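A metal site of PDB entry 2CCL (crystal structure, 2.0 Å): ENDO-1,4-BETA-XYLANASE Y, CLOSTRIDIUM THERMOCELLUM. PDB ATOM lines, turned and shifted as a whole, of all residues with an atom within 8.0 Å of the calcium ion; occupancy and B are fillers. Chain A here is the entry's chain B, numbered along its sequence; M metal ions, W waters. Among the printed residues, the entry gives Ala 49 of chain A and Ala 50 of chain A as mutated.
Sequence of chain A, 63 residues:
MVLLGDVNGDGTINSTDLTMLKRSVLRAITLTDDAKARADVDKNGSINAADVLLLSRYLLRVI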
ATOM      1  N   LEU A  21      16.174 -15.735  13.523  1.00  0.00           N
ATOM      2  CA  LEU A  21      17.194 -16.374  12.706  1.00  0.00           C
ATOM      3  C   LEU A  21      18.324 -15.424  12.314  1.00  0.00           C
ATOM      4  O   LEU A  21      19.501 -15.754  12.482  1.00  0.00           O
ATOM      5  CB  LEU A  21      16.567 -17.022  11.457  1.00  0.00           C
ATOM      6  CG  LEU A  21      17.487 -17.851  10.544  1.00  0.00           C
ATOM      7  CD1 LEU A  21      18.233 -18.941  11.309  1.00  0.00           C
ATOM      8  CD2 LEU A  21      16.671 -18.469   9.405  1.00  0.00           C
ATOM      9  N   LYS A  36      17.847 -24.584  17.168  1.00  0.00           N
ATOM     10  CA  LYS A  36      18.876 -24.784  16.131  1.00  0.00           C
ATOM     11  C   LYS A  36      18.432 -25.798  15.078  1.00  0.00           C
ATOM     12  O   LYS A  36      18.657 -25.604  13.885  1.00  0.00           O
ATOM     13  CB  LYS A  36      20.204 -25.224  16.761  1.00  0.00           C
ATOM     14  CG  LYS A  36      20.889 -24.146  17.606  1.00  0.00           C
ATOM     15  CD  LYS A  36      22.150 -24.701  18.266  1.00  0.00           C
ATOM     16  CE  LYS A  36      22.656 -23.768  19.357  1.00  0.00           C
ATOM     17  NZ  LYS A  36      23.859 -24.319  20.052  1.00  0.00           N
ATOM     18  N   ALA A  39      15.903 -24.091  12.981  1.00  0.00           N
ATOM     19  CA  ALA A  39      16.530 -22.981  12.239  1.00  0.00           C
ATOM     20  C   ALA A  39      17.274 -23.422  10.975  1.00  0.00           C
ATOM     21  O   ALA A  39      17.341 -22.670   9.992  1.00  0.00           O
ATOM     22  CB  ALA A  39      17.471 -22.203  13.147  1.00  0.00           C
ATOM     23  N   ASP A  40      17.829 -24.631  11.000  1.00  0.00           N
ATOM     24  CA  ASP A  40      18.564 -25.182   9.856  1.00  0.00           C
ATOM     25  C   ASP A  40      17.580 -25.639   8.783  1.00  0.00           C
ATOM     26  O   ASP A  40      17.339 -26.837   8.607  1.00  0.00           O
ATOM     27  CB  ASP A  40      19.465 -26.342  10.313  1.00  0.00           C
ATOM     28  CG  ASP A  40      20.411 -26.807   9.215  1.00  0.00           C
ATOM     29  OD1 ASP A  40      20.463 -26.175   8.132  1.00  0.00           O
ATOM     30  OD2 ASP A  40      21.105 -27.826   9.422  1.00  0.00           O
ATOM     31  N   VAL A  41      17.024 -24.660   8.074  1.00  0.00           N
ATOM     32  CA  VAL A  41      15.913 -24.903   7.154  1.00  0.00           C
ATOM     33  C   VAL A  41      16.266 -25.699   5.890  1.00  0.00           C
ATOM     34  O   VAL A  41      15.410 -26.375   5.334  1.00  0.00           O
ATOM     35  CB  VAL A  41      15.173 -23.586   6.781  1.00  0.00           C
ATOM     36  CG1 VAL A  41      14.423 -23.055   7.993  1.00  0.00           C
ATOM     37  CG2 VAL A  41      16.146 -22.542   6.249  1.00  0.00           C
ATOM     38  N   ASP A  42      17.540 -25.635   5.465  1.00  0.00           N
ATOM     39  CA  ASP A  42      17.999 -26.437   4.328  1.00  0.00           C
ATOM     40  C   ASP A  42      18.682 -27.737   4.757  1.00  0.00           C
ATOM     41  O   ASP A  42      19.116 -28.533   3.904  1.00  0.00           O
ATOM     42  CB  ASP A  42      18.875 -25.612   3.365  1.00  0.00           C
ATOM     43  CG  ASP A  42      20.123 -25.038   4.029  1.00  0.00           C
ATOM     44  OD1 ASP A  42      20.526 -25.517   5.107  1.00  0.00           O
ATOM     45  OD2 ASP A  42      20.699 -24.089   3.457  1.00  0.00           O
ATOM     46  N   LYS A  43      18.763 -27.933   6.076  1.00  0.00           N
ATOM     47  CA  LYS A  43      19.212 -29.188   6.706  1.00  0.00           C
ATOM     48  C   LYS A  43      20.621 -29.628   6.294  1.00  0.00           C
ATOM     49  O   LYS A  43      20.884 -30.824   6.136  1.00  0.00           O
ATOM     50  CB  LYS A  43      18.197 -30.313   6.470  1.00  0.00           C
ATOM     51  CG  LYS A  43      16.738 -29.897   6.678  1.00  0.00           C
ATOM     52  CD  LYS A  43      15.777 -31.003   6.324  1.00  0.00           C
ATOM     53  CE  LYS A  43      15.452 -31.876   7.528  1.00  0.00           C
ATOM     54  NZ  LYS A  43      14.249 -32.726   7.292  1.00  0.00           N
ATOM     55  N   ASN A  44      21.529 -28.669   6.138  1.00  0.00           N
ATOM     56  CA  ASN A  44      22.906 -28.980   5.750  1.00  0.00           C
ATOM     57  C   ASN A  44      23.885 -29.055   6.928  1.00  0.00           C
ATOM     58  O   ASN A  44      25.070 -29.330   6.722  1.00  0.00           O
ATOM     59  CB  ASN A  44      23.396 -27.998   4.671  1.00  0.00           C
ATOM     60  CG  ASN A  44      23.497 -26.566   5.165  1.00  0.00           C
ATOM     61  OD1 ASN A  44      23.188 -26.261   6.330  1.00  0.00           O
ATOM     62  ND2 ASN A  44      23.914 -25.676   4.282  1.00  0.00           N
ATOM     63  N   GLY A  45      23.385 -28.801   8.128  1.00  0.00           N
ATOM     64  CA  GLY A  45      24.181 -28.934   9.353  1.00  0.00           C
ATOM     65  C   GLY A  45      24.722 -27.634   9.906  1.00  0.00           C
ATOM     66  O   GLY A  45      25.367 -27.632  10.962  1.00  0.00           O
ATOM     67  N   SER A  46      24.444 -26.528   9.222  1.00  0.00           N
ATOM     68  CA  SER A  46      24.917 -25.212   9.618  1.00  0.00           C
ATOM     69  C   SER A  46      23.787 -24.184   9.623  1.00  0.00           C
ATOM     70  O   SER A  46      22.823 -24.299   8.865  1.00  0.00           O
ATOM     71  CB  SER A  46      26.029 -24.740   8.670  1.00  0.00           C
ATOM     72  OG  SER A  46      27.189 -25.556   8.782  1.00  0.00           O
ATOM     73  N   ILE A  47      23.916 -23.176  10.484  1.00  0.00           N
ATOM     74  CA  ILE A  47      22.989 -22.037  10.490  1.00  0.00           C
ATOM     75  C   ILE A  47      23.711 -20.826   9.926  1.00  0.00           C
ATOM     76  O   ILE A  47      24.679 -20.342  10.523  1.00  0.00           O
ATOM     77  CB  ILE A  47      22.476 -21.704  11.918  1.00  0.00           C
ATOM     78  CG1 ILE A  47      22.061 -22.962  12.691  1.00  0.00           C
ATOM     79  CG2 ILE A  47      21.372 -20.630  11.858  1.00  0.00           C
ATOM     80  CD1 ILE A  47      20.868 -23.688  12.135  1.00  0.00           C
ATOM     81  N   ASN A  48      23.244 -20.331   8.786  1.00  0.00           N
ATOM     82  CA  ASN A  48      23.907 -19.225   8.108  1.00  0.00           C
ATOM     83  C   ASN A  48      22.956 -18.346   7.286  1.00  0.00           C
ATOM     84  O   ASN A  48      21.738 -18.497   7.350  1.00  0.00           O
ATOM     85  CB  ASN A  48      25.063 -19.737   7.241  1.00  0.00           C
ATOM     86  CG  ASN A  48      24.623 -20.799   6.231  1.00  0.00           C
ATOM     87  OD1 ASN A  48      23.471 -20.823   5.793  1.00  0.00           O
ATOM     88  ND2 ASN A  48      25.555 -21.671   5.864  1.00  0.00           N
ATOM     89  N   ALA A  49      23.537 -17.423   6.517  1.00  0.00           N
ATOM     90  CA  ALA A  49      22.788 -16.512   5.653  1.00  0.00           C
ATOM     91  C   ALA A  49      21.893 -17.241   4.645  1.00  0.00           C
ATOM     92  O   ALA A  49      20.814 -16.755   4.301  1.00  0.00           O
ATOM     93  CB  ALA A  49      23.734 -15.558   4.923  1.00  0.00           C
ATOM     94  N   ALA A  50      22.343 -18.411   4.178  1.00  0.00           N
ATOM     95  CA  ALA A  50      21.556 -19.233   3.254  1.00  0.00           C
ATOM     96  C   ALA A  50      20.237 -19.708   3.878  1.00  0.00           C
ATOM     97  O   ALA A  50      19.219 -19.794   3.187  1.00  0.00           O
ATOM     98  CB  ALA A  50      22.377 -20.409   2.744  1.00  0.00           C
ATOM     99  N   ASP A  51      20.252 -19.991   5.185  1.00  0.00           N
ATOM    100  CA  ASP A  51      19.022 -20.311   5.912  1.00  0.00           C
ATOM    101  C   ASP A  51      18.070 -19.119   6.005  1.00  0.00           C
ATOM    102  O   ASP A  51      16.853 -19.277   5.860  1.00  0.00           O
ATOM    103  CB  ASP A  51      19.338 -20.833   7.318  1.00  0.00           C
ATOM    104  CG  ASP A  51      20.030 -22.169   7.300  1.00  0.00           C
ATOM    105  OD1 ASP A  51      19.445 -23.160   6.812  1.00  0.00           O
ATOM    106  OD2 ASP A  51      21.187 -22.246   7.769  1.00  0.00           O
ATOM    107  N   VAL A  52      18.641 -17.942   6.251  1.00  0.00           N
ATOM    108  CA  VAL A  52      17.878 -16.691   6.310  1.00  0.00           C
ATOM    109  C   VAL A  52      17.121 -16.467   4.993  1.00  0.00           C
ATOM    110  O   VAL A  52      15.928 -16.181   4.998  1.00  0.00           O
ATOM    111  CB  VAL A  52      18.792 -15.486   6.630  1.00  0.00           C
ATOM    112  CG1 VAL A  52      18.051 -14.165   6.435  1.00  0.00           C
ATOM    113  CG2 VAL A  52      19.337 -15.591   8.062  1.00  0.00           C
ATOM    114  N   LEU A  54      16.436 -18.698   2.582  1.00  0.00           N
ATOM    115  CA  LEU A  54      15.463 -19.756   2.350  1.00  0.00           C
ATOM    116  C   LEU A  54      14.165 -19.511   3.127  1.00  0.00           C
ATOM    117  O   LEU A  54      13.065 -19.644   2.579  1.00  0.00           O
ATOM    118  CB  LEU A  54      16.041 -21.132   2.672  1.00  0.00           C
ATOM    119  CG  LEU A  54      15.133 -22.343   2.374  1.00  0.00           C
ATOM    120  CD1 LEU A  54      14.750 -22.368   0.896  1.00  0.00           C
ATOM    121  CD2 LEU A  54      15.806 -23.639   2.759  1.00  0.00           C
HETATM  122 CA    CA M   1      21.653 -24.520   6.975  1.00  0.00          CA
HETATM  123  O   HOH W   1      22.696 -23.208   5.234  1.00  0.00           O
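O of Ser 46 binds the calcium ion. The side-chain carboxylate (OD1) of Asp 40 binds the calcium ion (2.3 Å). OD1 of Asp 42 binds the calcium ion (2.4 Å). The calcium ion is bound by OD1 of Asn 44 (2.4 Å). Water W1 is bound to the calcium ion. The calcium ion is bound by OD2 of Asp 51 (2.5 Å). OD1 of Asp 51 binds the calcium ion (2.6 Å).
OD1 of Asp 40 sits close to N of Lys 43. The side-chain carboxylate (OD1) of Asp 51 lies close to the backbone NH (N) of Val 41. The side-chain carboxylate (OD2) of Asp 40 is in hydrogen-bond range of the backbone NH (N) of Gly 45, 2.8 Å away. The side-chain amide oxygen (OD1) of Asn 48 lies within hydrogen-bond range of the backbone NH (N) of Asp 51 (3.4 Å).
Of the 17 residues printed, 5 come within 4 Å of the calcium ion.
Water W1 lies within hydrogen-bond range of the side-chain amide oxygen of Asn 48, the side-chain carboxylate of Asp 42 and the side-chain amide nitrogen of Asn 44.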
